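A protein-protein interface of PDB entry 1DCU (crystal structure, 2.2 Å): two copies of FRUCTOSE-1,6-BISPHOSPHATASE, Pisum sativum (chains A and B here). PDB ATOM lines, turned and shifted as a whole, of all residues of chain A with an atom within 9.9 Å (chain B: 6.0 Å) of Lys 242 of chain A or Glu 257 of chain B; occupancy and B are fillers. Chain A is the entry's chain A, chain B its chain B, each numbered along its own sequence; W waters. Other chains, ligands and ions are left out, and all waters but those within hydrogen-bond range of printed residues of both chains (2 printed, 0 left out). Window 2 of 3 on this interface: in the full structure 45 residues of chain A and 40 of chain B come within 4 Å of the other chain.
The side-chain amide oxygen of Asn 237 of chain A lies close to the backbone NH of Gly 239 of chain A (3.0 Å). The side-chain carboxylate (OE2) of Glu 238 of chain A lies within salt-bridge range of the side-chain amino group (NZ) of Lys 256 of chain A (3.1 Å). O of Leu 255 of chain B lies within hydrogen-bond range of N of Tyr 265 of chain B (3.0 Å).
Gly 239 of chain A touches Pro 264 of chain B. Lys 256 of chain B touches Lys 242 of chain A. Glu 257 of chain B touches Lys 242 of chain A (OE2 to CE, 3.0 Å).
The side-chain carboxylate (OE1) of Glu 238 of chain A is in salt-bridge range of the side-chain amino group (NZ) of Lys 256 of chain B, at 3.6 Å. The backbone carbonyl oxygen (O) of Tyr 265 of chain B sits close to the backbone carbonyl oxygen (O) of Gly 239 of chain A (3.4 Å).
Of the 10 printed residues of chain B, 4 touch a printed residue of chain A. Hydrophobic or aromatic side chains of chain B that line the printed part of chain A: Pro 264. Along chain B the printed residues that touch a printed residue of chain A span positions 256 to 265. Along chain A the printed residues that touch a printed residue of chain B span positions 238 to 242.
Printed residues of chain B within 4 Å of Glu 238 of chain A: Lys 256. Printed residues of chain B within 4 Å of Gly 239 of chain A: Pro 264 (3.1 Å) and Tyr 265 (3.2 Å). Printed residues of chain A within 4 Å of Lys 256 of chain B: Glu 238 and Lys 242. Glu 257 of chain B touches just one residue of chain A: Lys 242 (3.0 Å). No residue of chain A comes within 4 Å of Gly 259 of chain B. The nearest residue of chain B that does not touch Lys 242 of chain A is Pro 258 of chain B (4.7 Å). The nearest residue of chain A that does not touch Glu 257 of chain B is Gly 239 of chain A (5.8 Å).
Water W1 lies within hydrogen-bond range of O of Gly 239 of chain A, O of Lys 256 of chain B, N of Lys 242 of chain A and N of Tyr 241 of chain A. Water W2 lies within hydrogen-bond range of ND2 of Asn 240 of chain A (2.7 Å), O of Tyr 265 of chain B (2.8 Å) and ND2 of Asn 237 of chain A (3.3 Å).
Positions printed for both chains: 253 and 256. Of the 5 pairs that touch across the chains among the printed residues, none has its exchanged pair printed and touching as well.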
ATOM      1  N   ASN A 237     -16.305  18.798  16.949  1.00  0.00           N
ATOM      2  CA  ASN A 237     -15.421  19.879  16.576  1.00  0.00           C
ATOM      3  C   ASN A 237     -14.076  19.202  16.217  1.00  0.00           C
ATOM      4  O   ASN A 237     -13.203  19.079  17.096  1.00  0.00           O
ATOM      5  CB  ASN A 237     -15.270  20.828  17.819  1.00  0.00           C
ATOM      6  CG  ASN A 237     -14.274  21.913  17.362  1.00  0.00           C
ATOM      7  OD1 ASN A 237     -13.876  21.987  16.205  1.00  0.00           O
ATOM      8  ND2 ASN A 237     -13.966  22.800  18.292  1.00  0.00           N
ATOM      9  N   GLU A 238     -13.832  18.913  14.968  1.00  0.00           N
ATOM     10  CA  GLU A 238     -12.668  18.221  14.442  1.00  0.00           C
ATOM     11  C   GLU A 238     -11.438  19.121  14.518  1.00  0.00           C
ATOM     12  O   GLU A 238     -10.383  18.606  14.149  1.00  0.00           O
ATOM     13  CB  GLU A 238     -12.863  17.764  12.998  1.00  0.00           C
ATOM     14  CG  GLU A 238     -13.582  16.460  12.857  1.00  0.00           C
ATOM     15  CD  GLU A 238     -13.157  15.612  11.635  1.00  0.00           C
ATOM     16  OE1 GLU A 238     -12.015  15.146  11.524  1.00  0.00           O
ATOM     17  OE2 GLU A 238     -14.128  15.473  10.891  1.00  0.00           O
ATOM     18  N   GLY A 239     -11.661  20.422  14.832  1.00  0.00           N
ATOM     19  CA  GLY A 239     -10.489  21.277  15.003  1.00  0.00           C
ATOM     20  C   GLY A 239      -9.579  20.791  16.157  1.00  0.00           C
ATOM     21  O   GLY A 239      -8.435  21.236  16.263  1.00  0.00           O
ATOM     22  N   ASN A 240     -10.050  20.057  17.133  1.00  0.00           N
ATOM     23  CA  ASN A 240      -9.463  19.477  18.272  1.00  0.00           C
ATOM     24  C   ASN A 240      -8.954  18.045  17.962  1.00  0.00           C
ATOM     25  O   ASN A 240      -8.488  17.348  18.861  1.00  0.00           O
ATOM     26  CB  ASN A 240     -10.524  19.367  19.409  1.00  0.00           C
ATOM     27  CG  ASN A 240     -10.958  20.666  19.996  1.00  0.00           C
ATOM     28  OD1 ASN A 240     -12.040  20.811  20.648  1.00  0.00           O
ATOM     29  ND2 ASN A 240     -10.173  21.702  19.870  1.00  0.00           N
ATOM     30  N   TYR A 241      -8.951  17.565  16.715  1.00  0.00           N
ATOM     31  CA  TYR A 241      -8.559  16.198  16.451  1.00  0.00           C
ATOM     32  C   TYR A 241      -7.184  15.819  16.991  1.00  0.00           C
ATOM     33  O   TYR A 241      -7.066  14.774  17.584  1.00  0.00           O
ATOM     34  CB  TYR A 241      -8.712  15.931  14.983  1.00  0.00           C
ATOM     35  CG  TYR A 241      -8.085  14.664  14.436  1.00  0.00           C
ATOM     36  CD1 TYR A 241      -8.891  13.586  14.168  1.00  0.00           C
ATOM     37  CD2 TYR A 241      -6.750  14.543  14.109  1.00  0.00           C
ATOM     38  CE1 TYR A 241      -8.474  12.390  13.619  1.00  0.00           C
ATOM     39  CE2 TYR A 241      -6.249  13.365  13.569  1.00  0.00           C
ATOM     40  CZ  TYR A 241      -7.116  12.320  13.318  1.00  0.00           C
ATOM     41  OH  TYR A 241      -6.609  11.204  12.699  1.00  0.00           O
ATOM     42  N   LYS A 242      -6.207  16.708  16.973  1.00  0.00           N
ATOM     43  CA  LYS A 242      -4.873  16.455  17.459  1.00  0.00           C
ATOM     44  C   LYS A 242      -4.801  16.582  18.959  1.00  0.00           C
ATOM     45  O   LYS A 242      -3.729  16.502  19.552  1.00  0.00           O
ATOM     46  CB  LYS A 242      -3.864  17.389  16.763  1.00  0.00           C
ATOM     47  CG  LYS A 242      -3.598  17.046  15.302  1.00  0.00           C
ATOM     48  CD  LYS A 242      -2.220  17.508  14.859  1.00  0.00           C
ATOM     49  CE  LYS A 242      -1.439  16.503  14.024  1.00  0.00           C
ATOM     50  NZ  LYS A 242      -1.195  15.202  14.727  1.00  0.00           N
ATOM     51  N   LEU A 243      -5.914  16.849  19.638  1.00  0.00           N
ATOM     52  CA  LEU A 243      -5.905  16.929  21.085  1.00  0.00           C
ATOM     53  C   LEU A 243      -6.666  15.732  21.613  1.00  0.00           C
ATOM     54  O   LEU A 243      -6.995  15.712  22.810  1.00  0.00           O
ATOM     55  CB  LEU A 243      -6.518  18.215  21.574  1.00  0.00           C
ATOM     56  CG  LEU A 243      -6.251  19.538  20.866  1.00  0.00           C
ATOM     57  CD1 LEU A 243      -6.968  20.695  21.580  1.00  0.00           C
ATOM     58  CD2 LEU A 243      -4.746  19.806  20.813  1.00  0.00           C
ATOM     59  N   TRP A 244      -7.052  14.828  20.695  1.00  0.00           N
ATOM     60  CA  TRP A 244      -7.861  13.695  21.172  1.00  0.00           C
ATOM     61  C   TRP A 244      -6.964  12.450  21.413  1.00  0.00           C
ATOM     62  O   TRP A 244      -5.836  12.437  20.900  1.00  0.00           O
ATOM     63  CB  TRP A 244      -8.954  13.252  20.197  1.00  0.00           C
ATOM     64  CG  TRP A 244     -10.124  14.241  20.109  1.00  0.00           C
ATOM     65  CD1 TRP A 244     -10.586  15.111  21.040  1.00  0.00           C
ATOM     66  CD2 TRP A 244     -10.936  14.432  18.950  1.00  0.00           C
ATOM     67  NE1 TRP A 244     -11.655  15.836  20.598  1.00  0.00           N
ATOM     68  CE2 TRP A 244     -11.866  15.453  19.284  1.00  0.00           C
ATOM     69  CE3 TRP A 244     -10.971  13.924  17.664  1.00  0.00           C
ATOM     70  CZ2 TRP A 244     -12.784  15.913  18.350  1.00  0.00           C
ATOM     71  CZ3 TRP A 244     -11.915  14.348  16.727  1.00  0.00           C
ATOM     72  CH2 TRP A 244     -12.783  15.354  17.102  1.00  0.00           C
ATOM     73  N   ASP A 245      -7.557  11.431  22.035  1.00  0.00           N
ATOM     74  CA  ASP A 245      -6.824  10.181  22.222  1.00  0.00           C
ATOM     75  C   ASP A 245      -6.785   9.434  20.904  1.00  0.00           C
ATOM     76  O   ASP A 245      -7.731   9.641  20.108  1.00  0.00           O
ATOM     77  CB  ASP A 245      -7.598   9.325  23.240  1.00  0.00           C
ATOM     78  CG  ASP A 245      -7.528   9.871  24.651  1.00  0.00           C
ATOM     79  OD1 ASP A 245      -6.609  10.663  24.926  1.00  0.00           O
ATOM     80  OD2 ASP A 245      -8.362   9.502  25.513  1.00  0.00           O
ATOM     81  N   GLU A 246      -5.791   8.542  20.715  1.00  0.00           N
ATOM     82  CA  GLU A 246      -5.733   7.772  19.490  1.00  0.00           C
ATOM     83  C   GLU A 246      -6.946   6.901  19.261  1.00  0.00           C
ATOM     84  O   GLU A 246      -7.291   6.744  18.076  1.00  0.00           O
ATOM     85  CB  GLU A 246      -4.459   6.901  19.393  1.00  0.00           C
ATOM     86  CG  GLU A 246      -3.169   7.694  19.446  1.00  0.00           C
ATOM     87  CD  GLU A 246      -2.852   8.453  18.176  1.00  0.00           C
ATOM     88  OE1 GLU A 246      -3.121   7.957  17.056  1.00  0.00           O
ATOM     89  OE2 GLU A 246      -2.319   9.596  18.199  1.00  0.00           O
ATOM     90  N   LEU A 248     -10.023   7.643  19.760  1.00  0.00           N
ATOM     91  CA  LEU A 248     -11.064   8.523  19.250  1.00  0.00           C
ATOM     92  C   LEU A 248     -10.705   8.899  17.814  1.00  0.00           C
ATOM     93  O   LEU A 248     -11.542   8.647  16.924  1.00  0.00           O
ATOM     94  CB  LEU A 248     -11.244   9.732  20.150  1.00  0.00           C
ATOM     95  CG  LEU A 248     -12.374  10.699  19.726  1.00  0.00           C
ATOM     96  CD1 LEU A 248     -13.707  10.048  19.504  1.00  0.00           C
ATOM     97  CD2 LEU A 248     -12.359  11.804  20.802  1.00  0.00           C
ATOM     98  N   LYS A 249      -9.456   9.264  17.615  1.00  0.00           N
ATOM     99  CA  LYS A 249      -8.986   9.573  16.278  1.00  0.00           C
ATOM    100  C   LYS A 249      -9.224   8.460  15.262  1.00  0.00           C
ATOM    101  O   LYS A 249      -9.645   8.794  14.121  1.00  0.00           O
ATOM    102  CB  LYS A 249      -7.549  10.033  16.099  1.00  0.00           C
ATOM    103  CG  LYS A 249      -6.944  10.924  17.145  1.00  0.00           C
ATOM    104  CD  LYS A 249      -5.470  11.206  16.774  1.00  0.00           C
ATOM    105  CE  LYS A 249      -4.894  12.210  17.751  1.00  0.00           C
ATOM    106  NZ  LYS A 249      -3.498  12.614  17.356  1.00  0.00           N
ATOM    107  N   ILE A 252     -12.927   8.598  14.318  1.00  0.00           N
ATOM    108  CA  ILE A 252     -13.270   9.699  13.361  1.00  0.00           C
ATOM    109  C   ILE A 252     -12.759   9.363  11.966  1.00  0.00           C
ATOM    110  O   ILE A 252     -13.470   9.435  10.968  1.00  0.00           O
ATOM    111  CB  ILE A 252     -12.703  11.024  13.879  1.00  0.00           C
ATOM    112  CG1 ILE A 252     -13.310  11.348  15.258  1.00  0.00           C
ATOM    113  CG2 ILE A 252     -12.935  12.122  12.861  1.00  0.00           C
ATOM    114  CD1 ILE A 252     -14.783  11.605  15.391  1.00  0.00           C
ATOM    115  N   ASP A 253     -11.521   8.904  11.874  1.00  0.00           N
ATOM    116  CA  ASP A 253     -10.917   8.501  10.593  1.00  0.00           C
ATOM    117  C   ASP A 253     -11.731   7.465   9.846  1.00  0.00           C
ATOM    118  O   ASP A 253     -12.021   7.586   8.652  1.00  0.00           O
ATOM    119  CB  ASP A 253      -9.549   7.914  10.923  1.00  0.00           C
ATOM    120  CG  ASP A 253      -8.423   8.803  11.322  1.00  0.00           C
ATOM    121  OD1 ASP A 253      -8.370  10.047  11.354  1.00  0.00           O
ATOM    122  OD2 ASP A 253      -7.336   8.275  11.669  1.00  0.00           O
ATOM    123  N   LYS A 256     -15.079   8.592   7.740  1.00  0.00           N
ATOM    124  CA  LYS A 256     -14.692   9.197   6.493  1.00  0.00           C
ATOM    125  C   LYS A 256     -14.497   8.152   5.401  1.00  0.00           C
ATOM    126  O   LYS A 256     -14.667   8.488   4.233  1.00  0.00           O
ATOM    127  CB  LYS A 256     -13.385  10.012   6.692  1.00  0.00           C
ATOM    128  CG  LYS A 256     -13.633  11.130   7.710  1.00  0.00           C
ATOM    129  CD  LYS A 256     -12.524  12.141   7.921  1.00  0.00           C
ATOM    130  CE  LYS A 256     -12.927  12.964   9.144  1.00  0.00           C
ATOM    131  NZ  LYS A 256     -11.823  13.815   9.605  1.00  0.00           N
ATOM    132  N   ARG A 291     -13.445  14.413  25.934  1.00  0.00           N
ATOM    133  CA  ARG A 291     -12.373  15.115  26.675  1.00  0.00           C
ATOM    134  C   ARG A 291     -11.211  15.236  25.699  1.00  0.00           C
ATOM    135  O   ARG A 291     -11.107  14.439  24.768  1.00  0.00           O
ATOM    136  CB  ARG A 291     -11.884  14.384  27.902  1.00  0.00           C
ATOM    137  CG  ARG A 291     -11.178  13.089  27.584  1.00  0.00           C
ATOM    138  CD  ARG A 291     -10.632  12.428  28.858  1.00  0.00           C
ATOM    139  NE  ARG A 291      -9.998  11.181  28.374  1.00  0.00           N
ATOM    140  CZ  ARG A 291      -9.771  10.110  29.120  1.00  0.00           C
ATOM    141  NH1 ARG A 291     -10.116  10.093  30.411  1.00  0.00           N
ATOM    142  NH2 ARG A 291      -9.212   9.056  28.522  1.00  0.00           N
ATOM    143  N   ASP A 292     -10.312  16.162  25.953  1.00  0.00           N
ATOM    144  CA  ASP A 292      -9.127  16.325  25.098  1.00  0.00           C
ATOM    145  C   ASP A 292      -7.993  16.784  26.010  1.00  0.00           C
ATOM    146  O   ASP A 292      -8.225  17.029  27.206  1.00  0.00           O
ATOM    147  CB  ASP A 292      -9.454  17.317  24.001  1.00  0.00           C
ATOM    148  CG  ASP A 292      -9.966  18.648  24.484  1.00  0.00           C
ATOM    149  OD1 ASP A 292     -11.125  18.975  24.114  1.00  0.00           O
ATOM    150  OD2 ASP A 292      -9.318  19.448  25.210  1.00  0.00           O
ATOM    151  N   LYS A 293      -6.800  16.999  25.476  1.00  0.00           N
ATOM    152  CA  LYS A 293      -5.644  17.388  26.281  1.00  0.00           C
ATOM    153  C   LYS A 293      -5.848  18.684  27.056  1.00  0.00           C
ATOM    154  O   LYS A 293      -5.255  18.829  28.122  1.00  0.00           O
ATOM    155  CB  LYS A 293      -4.328  17.333  25.494  1.00  0.00           C
ATOM    156  CG  LYS A 293      -4.033  15.929  24.959  1.00  0.00           C
ATOM    157  CD  LYS A 293      -2.622  15.796  24.427  1.00  0.00           C
ATOM    158  CE  LYS A 293      -2.045  14.387  24.513  1.00  0.00           C
ATOM    159  NZ  LYS A 293      -0.561  14.377  24.341  1.00  0.00           N
ATOM    160  N   LYS A 294      -6.716  19.579  26.648  1.00  0.00           N
ATOM    161  CA  LYS A 294      -7.085  20.799  27.334  1.00  0.00           C
ATOM    162  C   LYS A 294      -8.298  20.652  28.249  1.00  0.00           C
ATOM    163  O   LYS A 294      -8.349  21.188  29.359  1.00  0.00           O
ATOM    164  CB  LYS A 294      -7.385  21.876  26.302  1.00  0.00           C
ATOM    165  N   ASP B 253      -5.274  19.254   7.303  1.00  0.00           N
ATOM    166  CA  ASP B 253      -4.474  18.624   8.356  1.00  0.00           C
ATOM    167  C   ASP B 253      -3.680  19.621   9.149  1.00  0.00           C
ATOM    168  O   ASP B 253      -3.804  19.509  10.384  1.00  0.00           O
ATOM    169  CB  ASP B 253      -3.431  17.660   7.757  1.00  0.00           C
ATOM    170  CG  ASP B 253      -4.030  16.430   7.156  1.00  0.00           C
ATOM    171  OD1 ASP B 253      -5.162  16.045   7.535  1.00  0.00           O
ATOM    172  OD2 ASP B 253      -3.365  15.816   6.292  1.00  0.00           O
ATOM    173  N   ASP B 254      -3.119  20.625   8.456  1.00  0.00           N
ATOM    174  CA  ASP B 254      -2.446  21.678   9.164  1.00  0.00           C
ATOM    175  C   ASP B 254      -3.308  22.632   9.951  1.00  0.00           C
ATOM    176  O   ASP B 254      -2.706  23.293  10.835  1.00  0.00           O
ATOM    177  CB  ASP B 254      -1.595  22.521   8.199  1.00  0.00           C
ATOM    178  CG  ASP B 254      -0.541  21.709   7.452  1.00  0.00           C
ATOM    179  OD1 ASP B 254      -0.083  20.608   7.887  1.00  0.00           O
ATOM    180  OD2 ASP B 254      -0.088  22.156   6.353  1.00  0.00           O
ATOM    181  N   LEU B 255      -4.634  22.696   9.730  1.00  0.00           N
ATOM    182  CA  LEU B 255      -5.441  23.661  10.510  1.00  0.00           C
ATOM    183  C   LEU B 255      -5.592  23.193  11.960  1.00  0.00           C
ATOM    184  O   LEU B 255      -5.730  23.934  12.933  1.00  0.00           O
ATOM    185  CB  LEU B 255      -6.844  23.829   9.906  1.00  0.00           C
ATOM    186  CG  LEU B 255      -6.878  24.481   8.508  1.00  0.00           C
ATOM    187  CD1 LEU B 255      -8.305  24.647   8.006  1.00  0.00           C
ATOM    188  CD2 LEU B 255      -6.064  25.757   8.627  1.00  0.00           C
ATOM    189  N   LYS B 256      -5.445  21.888  12.067  1.00  0.00           N
ATOM    190  CA  LYS B 256      -5.516  21.215  13.379  1.00  0.00           C
ATOM    191  C   LYS B 256      -4.278  21.210  14.242  1.00  0.00           C
ATOM    192  O   LYS B 256      -4.315  20.764  15.407  1.00  0.00           O
ATOM    193  CB  LYS B 256      -5.936  19.790  12.999  1.00  0.00           C
ATOM    194  CG  LYS B 256      -7.300  19.896  12.273  1.00  0.00           C
ATOM    195  CD  LYS B 256      -7.634  18.538  11.605  1.00  0.00           C
ATOM    196  CE  LYS B 256      -9.163  18.546  11.474  1.00  0.00           C
ATOM    197  NZ  LYS B 256      -9.541  17.505  10.496  1.00  0.00           N
ATOM    198  N   GLU B 257      -3.181  21.760  13.757  1.00  0.00           N
ATOM    199  CA  GLU B 257      -1.957  21.958  14.498  1.00  0.00           C
ATOM    200  C   GLU B 257      -2.069  23.184  15.398  1.00  0.00           C
ATOM    201  O   GLU B 257      -2.124  24.317  14.959  1.00  0.00           O
ATOM    202  CB  GLU B 257      -0.733  22.279  13.627  1.00  0.00           C
ATOM    203  CG  GLU B 257      -0.082  21.131  12.885  1.00  0.00           C
ATOM    204  CD  GLU B 257       0.447  20.102  13.877  1.00  0.00           C
ATOM    205  OE1 GLU B 257       0.993  20.470  14.941  1.00  0.00           O
ATOM    206  OE2 GLU B 257       0.240  18.915  13.537  1.00  0.00           O
ATOM    207  N   PRO B 258      -1.928  22.977  16.694  1.00  0.00           N
ATOM    208  CA  PRO B 258      -1.965  24.057  17.649  1.00  0.00           C
ATOM    209  C   PRO B 258      -0.932  25.133  17.391  1.00  0.00           C
ATOM    210  O   PRO B 258       0.237  24.840  17.136  1.00  0.00           O
ATOM    211  CB  PRO B 258      -1.676  23.368  18.966  1.00  0.00           C
ATOM    212  CG  PRO B 258      -1.703  21.920  18.754  1.00  0.00           C
ATOM    213  CD  PRO B 258      -1.870  21.622  17.302  1.00  0.00           C
ATOM    214  N   GLY B 259      -1.330  26.397  17.528  1.00  0.00           N
ATOM    215  CA  GLY B 259      -0.389  27.515  17.400  1.00  0.00           C
ATOM    216  C   GLY B 259       0.685  27.374  18.478  1.00  0.00           C
ATOM    217  O   GLY B 259       0.649  26.426  19.287  1.00  0.00           O
ATOM    218  N   LYS B 263      -3.520  26.733  20.495  1.00  0.00           N
ATOM    219  CA  LYS B 263      -4.899  26.480  20.032  1.00  0.00           C
ATOM    220  C   LYS B 263      -4.914  26.240  18.535  1.00  0.00           C
ATOM    221  O   LYS B 263      -4.451  27.011  17.712  1.00  0.00           O
ATOM    222  CB  LYS B 263      -5.821  27.583  20.504  1.00  0.00           C
ATOM    223  N   PRO B 264      -5.421  25.086  18.115  1.00  0.00           N
ATOM    224  CA  PRO B 264      -5.730  24.790  16.719  1.00  0.00           C
ATOM    225  C   PRO B 264      -6.956  25.571  16.184  1.00  0.00           C
ATOM    226  O   PRO B 264      -7.512  26.334  16.972  1.00  0.00           O
ATOM    227  CB  PRO B 264      -6.165  23.326  16.739  1.00  0.00           C
ATOM    228  CG  PRO B 264      -6.864  23.187  18.026  1.00  0.00           C
ATOM    229  CD  PRO B 264      -6.180  24.164  18.989  1.00  0.00           C
ATOM    230  N   TYR B 265      -7.292  25.485  14.899  1.00  0.00           N
ATOM    231  CA  TYR B 265      -8.518  26.123  14.413  1.00  0.00           C
ATOM    232  C   TYR B 265      -9.738  25.474  15.056  1.00  0.00           C
ATOM    233  O   TYR B 265      -9.718  24.359  15.567  1.00  0.00           O
ATOM    234  CB  TYR B 265      -8.614  25.908  12.900  1.00  0.00           C
ATOM    235  CG  TYR B 265      -7.826  26.952  12.135  1.00  0.00           C
ATOM    236  CD1 TYR B 265      -6.491  27.204  12.426  1.00  0.00           C
ATOM    237  CD2 TYR B 265      -8.432  27.695  11.126  1.00  0.00           C
ATOM    238  CE1 TYR B 265      -5.736  28.165  11.776  1.00  0.00           C
ATOM    239  CE2 TYR B 265      -7.678  28.612  10.429  1.00  0.00           C
ATOM    240  CZ  TYR B 265      -6.362  28.877  10.766  1.00  0.00           C
ATOM    241  OH  TYR B 265      -5.673  29.805  10.042  1.00  0.00           O
HETATM  242  O   HOH W   1      -6.324  19.772  16.854  1.00  0.00           O
HETATM  243  O   HOH W   2     -10.808  23.577  18.072  1.00  0.00           O
